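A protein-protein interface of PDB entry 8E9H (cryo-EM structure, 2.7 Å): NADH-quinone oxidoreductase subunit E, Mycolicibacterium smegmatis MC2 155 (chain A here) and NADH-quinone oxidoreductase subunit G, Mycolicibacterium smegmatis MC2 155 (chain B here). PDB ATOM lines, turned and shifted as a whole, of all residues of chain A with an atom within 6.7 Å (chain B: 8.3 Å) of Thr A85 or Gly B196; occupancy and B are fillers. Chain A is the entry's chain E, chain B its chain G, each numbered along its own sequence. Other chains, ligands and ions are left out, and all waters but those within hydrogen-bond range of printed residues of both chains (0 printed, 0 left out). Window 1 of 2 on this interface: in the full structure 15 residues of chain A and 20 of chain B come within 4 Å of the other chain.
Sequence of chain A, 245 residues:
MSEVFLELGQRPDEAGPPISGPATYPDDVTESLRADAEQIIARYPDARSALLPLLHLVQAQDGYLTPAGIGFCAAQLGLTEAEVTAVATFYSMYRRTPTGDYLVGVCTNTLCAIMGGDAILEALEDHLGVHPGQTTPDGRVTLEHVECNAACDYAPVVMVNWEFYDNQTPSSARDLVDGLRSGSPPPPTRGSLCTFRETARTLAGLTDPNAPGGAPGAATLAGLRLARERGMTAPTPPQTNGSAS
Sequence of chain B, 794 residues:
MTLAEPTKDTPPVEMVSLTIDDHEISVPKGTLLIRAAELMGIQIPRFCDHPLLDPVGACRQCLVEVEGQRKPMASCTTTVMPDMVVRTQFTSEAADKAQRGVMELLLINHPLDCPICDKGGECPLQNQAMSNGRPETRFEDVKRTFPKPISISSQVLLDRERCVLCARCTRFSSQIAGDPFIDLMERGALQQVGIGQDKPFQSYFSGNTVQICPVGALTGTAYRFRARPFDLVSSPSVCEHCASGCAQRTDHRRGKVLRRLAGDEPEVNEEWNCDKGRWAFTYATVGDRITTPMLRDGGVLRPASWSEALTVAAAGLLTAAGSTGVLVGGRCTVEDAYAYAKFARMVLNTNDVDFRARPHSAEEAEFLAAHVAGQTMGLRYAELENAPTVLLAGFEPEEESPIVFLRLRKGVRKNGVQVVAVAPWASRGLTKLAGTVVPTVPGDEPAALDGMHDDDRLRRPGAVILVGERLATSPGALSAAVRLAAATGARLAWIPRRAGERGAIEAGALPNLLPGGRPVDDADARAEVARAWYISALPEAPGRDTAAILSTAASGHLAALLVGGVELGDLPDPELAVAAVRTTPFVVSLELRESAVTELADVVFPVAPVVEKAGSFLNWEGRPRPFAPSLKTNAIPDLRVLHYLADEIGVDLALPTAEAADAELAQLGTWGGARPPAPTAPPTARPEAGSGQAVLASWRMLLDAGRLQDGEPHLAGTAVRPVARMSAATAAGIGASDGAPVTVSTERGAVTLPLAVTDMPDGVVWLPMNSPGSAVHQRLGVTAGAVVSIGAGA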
ATOM      1  N   GLY A   9     -24.135  -2.592 -23.748  1.00  0.00           N
ATOM      2  CA  GLY A   9     -23.478  -3.877 -23.732  1.00  0.00           C
ATOM      3  C   GLY A   9     -21.992  -3.791 -23.447  1.00  0.00           C
ATOM      4  O   GLY A   9     -21.446  -2.754 -23.065  1.00  0.00           O
ATOM      5  N   GLN A  10     -21.331  -4.927 -23.652  1.00  0.00           N
ATOM      6  CA  GLN A  10     -19.909  -5.035 -23.361  1.00  0.00           C
ATOM      7  C   GLN A  10     -19.099  -4.132 -24.279  1.00  0.00           C
ATOM      8  O   GLN A  10     -19.461  -3.907 -25.436  1.00  0.00           O
ATOM      9  CB  GLN A  10     -19.451  -6.482 -23.526  1.00  0.00           C
ATOM     10  CG  GLN A  10     -20.256  -7.479 -22.728  1.00  0.00           C
ATOM     11  CD  GLN A  10     -19.609  -8.847 -22.695  1.00  0.00           C
ATOM     12  OE1 GLN A  10     -18.438  -8.984 -22.349  1.00  0.00           O
ATOM     13  NE2 GLN A  10     -20.373  -9.870 -23.058  1.00  0.00           N
ATOM     14  N   ILE A  19     -19.169 -11.254 -28.480  1.00  0.00           N
ATOM     15  CA  ILE A  19     -19.723 -11.559 -29.790  1.00  0.00           C
ATOM     16  C   ILE A  19     -19.787 -10.284 -30.608  1.00  0.00           C
ATOM     17  O   ILE A  19     -20.327  -9.268 -30.159  1.00  0.00           O
ATOM     18  CB  ILE A  19     -21.113 -12.205 -29.646  1.00  0.00           C
ATOM     19  CG1 ILE A  19     -21.044 -13.470 -28.786  1.00  0.00           C
ATOM     20  CG2 ILE A  19     -21.688 -12.518 -31.011  1.00  0.00           C
ATOM     21  CD1 ILE A  19     -20.247 -14.595 -29.399  1.00  0.00           C
ATOM     22  N   LEU A  51     -30.331 -25.917 -29.549  1.00  0.00           N
ATOM     23  CA  LEU A  51     -29.590 -24.660 -29.562  1.00  0.00           C
ATOM     24  C   LEU A  51     -28.099 -24.890 -29.758  1.00  0.00           C
ATOM     25  O   LEU A  51     -27.457 -24.187 -30.546  1.00  0.00           O
ATOM     26  CB  LEU A  51     -29.841 -23.887 -28.271  1.00  0.00           C
ATOM     27  CG  LEU A  51     -29.058 -22.582 -28.144  1.00  0.00           C
ATOM     28  CD1 LEU A  51     -29.249 -21.711 -29.364  1.00  0.00           C
ATOM     29  CD2 LEU A  51     -29.491 -21.838 -26.906  1.00  0.00           C
ATOM     30  N   LEU A  55     -25.921 -23.383 -32.776  1.00  0.00           N
ATOM     31  CA  LEU A  55     -24.761 -22.522 -32.594  1.00  0.00           C
ATOM     32  C   LEU A  55     -23.568 -23.045 -33.377  1.00  0.00           C
ATOM     33  O   LEU A  55     -22.792 -22.261 -33.933  1.00  0.00           O
ATOM     34  CB  LEU A  55     -24.426 -22.397 -31.112  1.00  0.00           C
ATOM     35  CG  LEU A  55     -25.379 -21.488 -30.337  1.00  0.00           C
ATOM     36  CD1 LEU A  55     -25.212 -21.689 -28.847  1.00  0.00           C
ATOM     37  CD2 LEU A  55     -25.143 -20.038 -30.708  1.00  0.00           C
ATOM     38  N   ILE A  70     -26.235 -15.373 -33.671  1.00  0.00           N
ATOM     39  CA  ILE A  70     -27.008 -15.323 -32.436  1.00  0.00           C
ATOM     40  C   ILE A  70     -28.457 -14.981 -32.746  1.00  0.00           C
ATOM     41  O   ILE A  70     -29.388 -15.615 -32.240  1.00  0.00           O
ATOM     42  CB  ILE A  70     -26.391 -14.308 -31.459  1.00  0.00           C
ATOM     43  CG1 ILE A  70     -24.978 -14.733 -31.055  1.00  0.00           C
ATOM     44  CG2 ILE A  70     -27.271 -14.152 -30.237  1.00  0.00           C
ATOM     45  CD1 ILE A  70     -24.914 -16.006 -30.248  1.00  0.00           C
ATOM     46  N   THR A  80     -34.788 -14.952 -26.784  1.00  0.00           N
ATOM     47  CA  THR A  80     -34.193 -13.638 -26.936  1.00  0.00           C
ATOM     48  C   THR A  80     -32.709 -13.777 -27.243  1.00  0.00           C
ATOM     49  O   THR A  80     -32.062 -14.763 -26.880  1.00  0.00           O
ATOM     50  CB  THR A  80     -34.383 -12.801 -25.673  1.00  0.00           C
ATOM     51  OG1 THR A  80     -33.465 -13.238 -24.666  1.00  0.00           O
ATOM     52  CG2 THR A  80     -35.799 -12.929 -25.152  1.00  0.00           C
ATOM     53  N   GLU A  81     -32.163 -12.771 -27.924  1.00  0.00           N
ATOM     54  CA  GLU A  81     -30.739 -12.801 -28.227  1.00  0.00           C
ATOM     55  C   GLU A  81     -29.912 -12.914 -26.956  1.00  0.00           C
ATOM     56  O   GLU A  81     -28.797 -13.440 -26.986  1.00  0.00           O
ATOM     57  CB  GLU A  81     -30.344 -11.554 -29.014  1.00  0.00           C
ATOM     58  N   ALA A  82     -30.445 -12.439 -25.830  1.00  0.00           N
ATOM     59  CA  ALA A  82     -29.716 -12.535 -24.570  1.00  0.00           C
ATOM     60  C   ALA A  82     -29.559 -13.984 -24.132  1.00  0.00           C
ATOM     61  O   ALA A  82     -28.474 -14.403 -23.722  1.00  0.00           O
ATOM     62  CB  ALA A  82     -30.430 -11.724 -23.492  1.00  0.00           C
ATOM     63  N   GLU A  83     -30.633 -14.770 -24.202  1.00  0.00           N
ATOM     64  CA  GLU A  83     -30.538 -16.171 -23.804  1.00  0.00           C
ATOM     65  C   GLU A  83     -29.575 -16.927 -24.708  1.00  0.00           C
ATOM     66  O   GLU A  83     -28.751 -17.723 -24.235  1.00  0.00           O
ATOM     67  CB  GLU A  83     -31.922 -16.812 -23.838  1.00  0.00           C
ATOM     68  CG  GLU A  83     -32.905 -16.191 -22.865  1.00  0.00           C
ATOM     69  CD  GLU A  83     -34.270 -16.846 -22.915  1.00  0.00           C
ATOM     70  OE1 GLU A  83     -35.063 -16.498 -23.812  1.00  0.00           O
ATOM     71  OE2 GLU A  83     -34.552 -17.704 -22.055  1.00  0.00           O
ATOM     72  N   VAL A  84     -29.662 -16.688 -26.014  1.00  0.00           N
ATOM     73  CA  VAL A  84     -28.768 -17.362 -26.941  1.00  0.00           C
ATOM     74  C   VAL A  84     -27.327 -16.971 -26.661  1.00  0.00           C
ATOM     75  O   VAL A  84     -26.428 -17.812 -26.701  1.00  0.00           O
ATOM     76  CB  VAL A  84     -29.167 -17.046 -28.391  1.00  0.00           C
ATOM     77  CG1 VAL A  84     -28.181 -17.670 -29.354  1.00  0.00           C
ATOM     78  CG2 VAL A  84     -30.567 -17.540 -28.665  1.00  0.00           C
ATOM     79  N   THR A  85     -27.080 -15.691 -26.387  1.00  0.00           N
ATOM     80  CA  THR A  85     -25.721 -15.259 -26.085  1.00  0.00           C
ATOM     81  C   THR A  85     -25.223 -15.894 -24.797  1.00  0.00           C
ATOM     82  O   THR A  85     -24.047 -16.260 -24.689  1.00  0.00           O
ATOM     83  CB  THR A  85     -25.663 -13.739 -25.982  1.00  0.00           C
ATOM     84  OG1 THR A  85     -26.337 -13.155 -27.102  1.00  0.00           O
ATOM     85  CG2 THR A  85     -24.227 -13.262 -25.955  1.00  0.00           C
ATOM     86  N   ALA A  86     -26.096 -16.018 -23.802  1.00  0.00           N
ATOM     87  CA  ALA A  86     -25.699 -16.653 -22.554  1.00  0.00           C
ATOM     88  C   ALA A  86     -25.288 -18.095 -22.790  1.00  0.00           C
ATOM     89  O   ALA A  86     -24.286 -18.562 -22.240  1.00  0.00           O
ATOM     90  CB  ALA A  86     -26.841 -16.584 -21.547  1.00  0.00           C
ATOM     91  N   VAL A  87     -26.052 -18.818 -23.602  1.00  0.00           N
ATOM     92  CA  VAL A  87     -25.679 -20.192 -23.921  1.00  0.00           C
ATOM     93  C   VAL A  87     -24.375 -20.220 -24.706  1.00  0.00           C
ATOM     94  O   VAL A  87     -23.486 -21.034 -24.438  1.00  0.00           O
ATOM     95  CB  VAL A  87     -26.811 -20.890 -24.690  1.00  0.00           C
ATOM     96  CG1 VAL A  87     -26.375 -22.275 -25.111  1.00  0.00           C
ATOM     97  CG2 VAL A  87     -28.052 -20.956 -23.830  1.00  0.00           C
ATOM     98  N   ALA A  88     -24.240 -19.328 -25.685  1.00  0.00           N
ATOM     99  CA  ALA A  88     -23.098 -19.375 -26.587  1.00  0.00           C
ATOM    100  C   ALA A  88     -21.798 -19.069 -25.865  1.00  0.00           C
ATOM    101  O   ALA A  88     -20.824 -19.819 -25.982  1.00  0.00           O
ATOM    102  CB  ALA A  88     -23.308 -18.391 -27.734  1.00  0.00           C
ATOM    103  N   THR A  89     -21.758 -17.975 -25.111  1.00  0.00           N
ATOM    104  CA  THR A  89     -20.533 -17.570 -24.441  1.00  0.00           C
ATOM    105  C   THR A  89     -20.089 -18.561 -23.379  1.00  0.00           C
ATOM    106  O   THR A  89     -18.952 -18.473 -22.910  1.00  0.00           O
ATOM    107  CB  THR A  89     -20.716 -16.196 -23.799  1.00  0.00           C
ATOM    108  OG1 THR A  89     -21.822 -16.235 -22.892  1.00  0.00           O
ATOM    109  CG2 THR A  89     -20.975 -15.145 -24.858  1.00  0.00           C
ATOM    110  N   PHE A  90     -20.953 -19.494 -22.988  1.00  0.00           N
ATOM    111  CA  PHE A  90     -20.609 -20.427 -21.928  1.00  0.00           C
ATOM    112  C   PHE A  90     -19.649 -21.509 -22.397  1.00  0.00           C
ATOM    113  O   PHE A  90     -18.849 -22.005 -21.599  1.00  0.00           O
ATOM    114  CB  PHE A  90     -21.877 -21.070 -21.375  1.00  0.00           C
ATOM    115  CG  PHE A  90     -21.632 -21.987 -20.224  1.00  0.00           C
ATOM    116  CD1 PHE A  90     -21.470 -21.485 -18.951  1.00  0.00           C
ATOM    117  CD2 PHE A  90     -21.570 -23.351 -20.411  1.00  0.00           C
ATOM    118  CE1 PHE A  90     -21.250 -22.324 -17.890  1.00  0.00           C
ATOM    119  CE2 PHE A  90     -21.348 -24.194 -19.351  1.00  0.00           C
ATOM    120  CZ  PHE A  90     -21.189 -23.681 -18.090  1.00  0.00           C
ATOM    121  N   ILE B 152     -26.913  -1.293 -19.870  1.00  0.00           N
ATOM    122  CA  ILE B 152     -27.749  -2.337 -20.439  1.00  0.00           C
ATOM    123  C   ILE B 152     -29.079  -1.794 -20.938  1.00  0.00           C
ATOM    124  O   ILE B 152     -29.799  -2.519 -21.641  1.00  0.00           O
ATOM    125  CB  ILE B 152     -27.984  -3.477 -19.428  1.00  0.00           C
ATOM    126  CG1 ILE B 152     -28.595  -2.938 -18.139  1.00  0.00           C
ATOM    127  CG2 ILE B 152     -26.679  -4.176 -19.123  1.00  0.00           C
ATOM    128  CD1 ILE B 152     -29.208  -4.007 -17.277  1.00  0.00           C
ATOM    129  N   PRO B 180     -36.479 -12.040 -20.465  1.00  0.00           N
ATOM    130  CA  PRO B 180     -35.089 -12.479 -20.300  1.00  0.00           C
ATOM    131  C   PRO B 180     -34.126 -11.818 -21.282  1.00  0.00           C
ATOM    132  O   PRO B 180     -33.439 -12.486 -22.052  1.00  0.00           O
ATOM    133  CB  PRO B 180     -35.187 -13.989 -20.528  1.00  0.00           C
ATOM    134  CG  PRO B 180     -36.297 -14.127 -21.491  1.00  0.00           C
ATOM    135  CD  PRO B 180     -37.299 -13.072 -21.121  1.00  0.00           C
ATOM    136  N   PHE B 181     -34.083 -10.488 -21.260  1.00  0.00           N
ATOM    137  CA  PHE B 181     -33.150  -9.755 -22.101  1.00  0.00           C
ATOM    138  C   PHE B 181     -31.800  -9.549 -21.436  1.00  0.00           C
ATOM    139  O   PHE B 181     -30.880  -9.044 -22.087  1.00  0.00           O
ATOM    140  CB  PHE B 181     -33.748  -8.407 -22.492  1.00  0.00           C
ATOM    141  CG  PHE B 181     -35.032  -8.525 -23.243  1.00  0.00           C
ATOM    142  CD1 PHE B 181     -35.033  -8.787 -24.597  1.00  0.00           C
ATOM    143  CD2 PHE B 181     -36.240  -8.387 -22.595  1.00  0.00           C
ATOM    144  CE1 PHE B 181     -36.212  -8.901 -25.287  1.00  0.00           C
ATOM    145  CE2 PHE B 181     -37.423  -8.500 -23.282  1.00  0.00           C
ATOM    146  CZ  PHE B 181     -37.409  -8.757 -24.629  1.00  0.00           C
ATOM    147  N   ILE B 182     -31.662  -9.920 -20.169  1.00  0.00           N
ATOM    148  CA  ILE B 182     -30.379  -9.971 -19.486  1.00  0.00           C
ATOM    149  C   ILE B 182     -30.173 -11.395 -19.006  1.00  0.00           C
ATOM    150  O   ILE B 182     -31.124 -12.057 -18.577  1.00  0.00           O
ATOM    151  CB  ILE B 182     -30.307  -8.982 -18.307  1.00  0.00           C
ATOM    152  CG1 ILE B 182     -31.492  -9.180 -17.367  1.00  0.00           C
ATOM    153  CG2 ILE B 182     -30.279  -7.561 -18.814  1.00  0.00           C
ATOM    154  CD1 ILE B 182     -31.306  -8.522 -16.030  1.00  0.00           C
ATOM    155  N   ASP B 183     -28.940 -11.876 -19.092  1.00  0.00           N
ATOM    156  CA  ASP B 183     -28.649 -13.223 -18.632  1.00  0.00           C
ATOM    157  C   ASP B 183     -27.176 -13.311 -18.274  1.00  0.00           C
ATOM    158  O   ASP B 183     -26.384 -12.427 -18.598  1.00  0.00           O
ATOM    159  CB  ASP B 183     -29.031 -14.261 -19.684  1.00  0.00           C
ATOM    160  CG  ASP B 183     -29.182 -15.647 -19.101  1.00  0.00           C
ATOM    161  OD1 ASP B 183     -28.704 -15.865 -17.968  1.00  0.00           O
ATOM    162  OD2 ASP B 183     -29.783 -16.514 -19.765  1.00  0.00           O
ATOM    163  N   LEU B 184     -26.823 -14.391 -17.587  1.00  0.00           N
ATOM    164  CA  LEU B 184     -25.453 -14.597 -17.146  1.00  0.00           C
ATOM    165  C   LEU B 184     -24.607 -15.078 -18.315  1.00  0.00           C
ATOM    166  O   LEU B 184     -24.727 -16.227 -18.749  1.00  0.00           O
ATOM    167  CB  LEU B 184     -25.416 -15.597 -15.998  1.00  0.00           C
ATOM    168  CG  LEU B 184     -26.174 -15.172 -14.741  1.00  0.00           C
ATOM    169  CD1 LEU B 184     -25.964 -16.190 -13.646  1.00  0.00           C
ATOM    170  CD2 LEU B 184     -25.736 -13.802 -14.273  1.00  0.00           C
ATOM    171  N   MET B 185     -23.758 -14.196 -18.821  1.00  0.00           N
ATOM    172  CA  MET B 185     -22.913 -14.434 -19.970  1.00  0.00           C
ATOM    173  C   MET B 185     -21.584 -15.015 -19.501  1.00  0.00           C
ATOM    174  O   MET B 185     -21.230 -14.944 -18.321  1.00  0.00           O
ATOM    175  CB  MET B 185     -22.671 -13.118 -20.701  1.00  0.00           C
ATOM    176  CG  MET B 185     -23.922 -12.498 -21.278  1.00  0.00           C
ATOM    177  SD  MET B 185     -24.783 -13.406 -22.554  1.00  0.00           S
ATOM    178  CE  MET B 185     -26.241 -12.375 -22.672  1.00  0.00           C
ATOM    179  N   GLU B 186     -20.828 -15.570 -20.445  1.00  0.00           N
ATOM    180  CA  GLU B 186     -19.483 -16.057 -20.164  1.00  0.00           C
ATOM    181  C   GLU B 186     -19.506 -17.195 -19.154  1.00  0.00           C
ATOM    182  O   GLU B 186     -20.575 -17.704 -18.807  1.00  0.00           O
ATOM    183  CB  GLU B 186     -18.599 -14.920 -19.652  1.00  0.00           C
ATOM    184  CG  GLU B 186     -18.508 -13.735 -20.586  1.00  0.00           C
ATOM    185  CD  GLU B 186     -17.731 -14.048 -21.844  1.00  0.00           C
ATOM    186  OE1 GLU B 186     -17.101 -15.123 -21.901  1.00  0.00           O
ATOM    187  OE2 GLU B 186     -17.744 -13.216 -22.775  1.00  0.00           O
ATOM    188  N   VAL B 193     -23.419 -10.753 -15.740  1.00  0.00           N
ATOM    189  CA  VAL B 193     -24.731 -10.416 -16.270  1.00  0.00           C
ATOM    190  C   VAL B 193     -24.557  -9.504 -17.476  1.00  0.00           C
ATOM    191  O   VAL B 193     -23.683  -8.630 -17.500  1.00  0.00           O
ATOM    192  CB  VAL B 193     -25.607  -9.755 -15.194  1.00  0.00           C
ATOM    193  CG1 VAL B 193     -25.002  -8.450 -14.754  1.00  0.00           C
ATOM    194  CG2 VAL B 193     -27.004  -9.529 -15.729  1.00  0.00           C
ATOM    195  N   GLY B 194     -25.381  -9.712 -18.497  1.00  0.00           N
ATOM    196  CA  GLY B 194     -25.272  -8.894 -19.688  1.00  0.00           C
ATOM    197  C   GLY B 194     -26.452  -9.053 -20.614  1.00  0.00           C
ATOM    198  O   GLY B 194     -27.189 -10.042 -20.563  1.00  0.00           O
ATOM    199  N   ILE B 195     -26.627  -8.039 -21.461  1.00  0.00           N
ATOM    200  CA  ILE B 195     -27.575  -8.065 -22.569  1.00  0.00           C
ATOM    201  C   ILE B 195     -26.913  -8.789 -23.729  1.00  0.00           C
ATOM    202  O   ILE B 195     -25.705  -9.048 -23.694  1.00  0.00           O
ATOM    203  CB  ILE B 195     -28.010  -6.647 -22.971  1.00  0.00           C
ATOM    204  CG1 ILE B 195     -26.790  -5.779 -23.279  1.00  0.00           C
ATOM    205  CG2 ILE B 195     -28.829  -6.021 -21.867  1.00  0.00           C
ATOM    206  CD1 ILE B 195     -27.126  -4.502 -23.993  1.00  0.00           C
ATOM    207  N   GLY B 196     -27.679  -9.115 -24.765  1.00  0.00           N
ATOM    208  CA  GLY B 196     -27.131  -9.964 -25.801  1.00  0.00           C
ATOM    209  C   GLY B 196     -25.930  -9.363 -26.501  1.00  0.00           C
ATOM    210  O   GLY B 196     -24.799  -9.779 -26.239  1.00  0.00           O
ATOM    211  N   GLN B 197     -26.141  -8.392 -27.388  1.00  0.00           N
ATOM    212  CA  GLN B 197     -25.024  -7.603 -27.896  1.00  0.00           C
ATOM    213  C   GLN B 197     -25.286  -6.120 -27.701  1.00  0.00           C
ATOM    214  O   GLN B 197     -24.502  -5.411 -27.064  1.00  0.00           O
ATOM    215  CB  GLN B 197     -24.782  -7.911 -29.371  1.00  0.00           C
ATOM    216  CG  GLN B 197     -24.167  -9.271 -29.597  1.00  0.00           C
ATOM    217  CD  GLN B 197     -25.162 -10.389 -29.399  1.00  0.00           C
ATOM    218  OE1 GLN B 197     -26.297 -10.314 -29.865  1.00  0.00           O
ATOM    219  NE2 GLN B 197     -24.748 -11.428 -28.688  1.00  0.00           N
ATOM    220  N   ASP B 198     -26.401  -5.656 -28.259  1.00  0.00           N
ATOM    221  CA  ASP B 198     -26.818  -4.270 -28.112  1.00  0.00           C
ATOM    222  C   ASP B 198     -28.303  -4.171 -27.806  1.00  0.00           C
ATOM    223  O   ASP B 198     -28.766  -3.128 -27.332  1.00  0.00           O
ATOM    224  CB  ASP B 198     -26.488  -3.485 -29.381  1.00  0.00           C
ATOM    225  N   LYS B 199     -29.059  -5.233 -28.081  1.00  0.00           N
ATOM    226  CA  LYS B 199     -30.476  -5.273 -27.763  1.00  0.00           C
ATOM    227  C   LYS B 199     -30.658  -4.868 -26.307  1.00  0.00           C
ATOM    228  O   LYS B 199     -30.282  -5.623 -25.403  1.00  0.00           O
ATOM    229  CB  LYS B 199     -31.046  -6.668 -28.016  1.00  0.00           C
ATOM    230  N   PRO B 200     -31.223  -3.697 -26.035  1.00  0.00           N
ATOM    231  CA  PRO B 200     -31.266  -3.206 -24.658  1.00  0.00           C
ATOM    232  C   PRO B 200     -32.189  -4.046 -23.793  1.00  0.00           C
ATOM    233  O   PRO B 200     -33.086  -4.739 -24.272  1.00  0.00           O
ATOM    234  CB  PRO B 200     -31.799  -1.781 -24.809  1.00  0.00           C
ATOM    235  CG  PRO B 200     -32.623  -1.834 -26.034  1.00  0.00           C
ATOM    236  CD  PRO B 200     -31.946  -2.801 -26.953  1.00  0.00           C
ATOM    237  N   PHE B 201     -31.950  -3.973 -22.489  1.00  0.00           N
ATOM    238  CA  PHE B 201     -32.847  -4.599 -21.533  1.00  0.00           C
ATOM    239  C   PHE B 201     -34.200  -3.909 -21.618  1.00  0.00           C
ATOM    240  O   PHE B 201     -34.366  -2.786 -21.132  1.00  0.00           O
ATOM    241  CB  PHE B 201     -32.255  -4.492 -20.130  1.00  0.00           C
ATOM    242  CG  PHE B 201     -33.047  -5.193 -19.070  1.00  0.00           C
ATOM    243  CD1 PHE B 201     -33.955  -6.181 -19.390  1.00  0.00           C
ATOM    244  CD2 PHE B 201     -32.865  -4.868 -17.742  1.00  0.00           C
ATOM    245  CE1 PHE B 201     -34.672  -6.821 -18.407  1.00  0.00           C
ATOM    246  CE2 PHE B 201     -33.578  -5.505 -16.758  1.00  0.00           C
ATOM    247  CZ  PHE B 201     -34.483  -6.483 -17.090  1.00  0.00           C
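The backbone NH of Ala A86 lies within hydrogen-bond range of the side-chain sulfur of Met B185, 3.2 Å away. The side-chain amide nitrogen (NE2) of Gln B197 sits at hydrogen-bond distance from the side-chain hydroxyl (OG1) of Thr A85, at 2.8 Å. The backbone carbonyl oxygen of Pro B180 sits at hydrogen-bond distance from the side-chain hydroxyl of Thr A80 (2.7 Å). The side-chain hydroxyl of Thr A89 is in hydrogen-bond range of the backbone NH of Glu B186 (2.7 Å). The backbone carbonyl oxygen (O) of Thr A85 sits close to the side-chain sulfur (SD) of Met B185.
The backbone NH (N) of Ala A82 sits close to the side-chain hydroxyl (OG1) of Thr A80 (3.3 Å). The backbone carbonyl oxygen (O) of Glu A81 lies within hydrogen-bond range of the side-chain hydroxyl (OG1) of Thr A85 (2.5 Å). N of Glu A83 sits at hydrogen-bond distance from OG1 of Thr A80. The backbone carbonyl oxygen (O) of Ala A86 lies within hydrogen-bond range of the side-chain hydroxyl (OG1) of Thr A89 (3.5 Å). The backbone carbonyl oxygen (O) of Asp B183 sits at hydrogen-bond distance from the backbone NH (N) of Gly B194, 2.9 Å away. The backbone carbonyl oxygen (O) of Thr A85 lies within hydrogen-bond range of the side-chain hydroxyl (OG1) of Thr A89.
Among the printed residues, pairs that only touch across the chains: Ala A82 with Phe B181, Ala A82 with Met B185, Ala A82 with Pro B180, Ala A86 with Asp B183, Ala A86 with Leu B184, Thr A85 with Gly B196, Glu A83 with Pro B180, Gly A9 with Ile B195, Thr A89 with Met B185, Gly A9 with Gln B197, Ile A19 with Gln B197, Ala A82 with Gly B196, Phe A90 with Glu B186, Ala A82 with Ile B182 and Ile A70 with Gln B197.
Thr A85 touches three residues of chain B. Of chain A, only Ala A82 (3.8 Å) and Thr A85 (3.5 Å) come within 4 Å of Gly B196. Ala A82 touches just these residues of chain B: Pro B180 (3.4 Å), Phe B181 (3.1 Å), Ile B182 (3.98 Å), Met B185 (3.2 Å) and Gly B196 (3.8 Å). Of the printed residues of chain A, Phe B181 touches Ala A82. Of the printed residues of chain B, Ile A19 touches Gln B197 (3.8 Å). Of the printed residues of chain A, Leu B184 touches Ala A86 (3.5 Å). Glu A81 touches none of the printed residues of chain B. Val A84 touches none of the printed residues of chain B. The nearest residue of chain B that does not touch Thr A85 is Ile B195 (5.0 Å). The nearest residue of chain A that does not touch Gly B196 is Glu A81 (4.03 Å).
Of the 17 printed residues of chain B, 10 touch a printed residue of chain A. Among the printed residues, 20 pairs touch across the chains.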
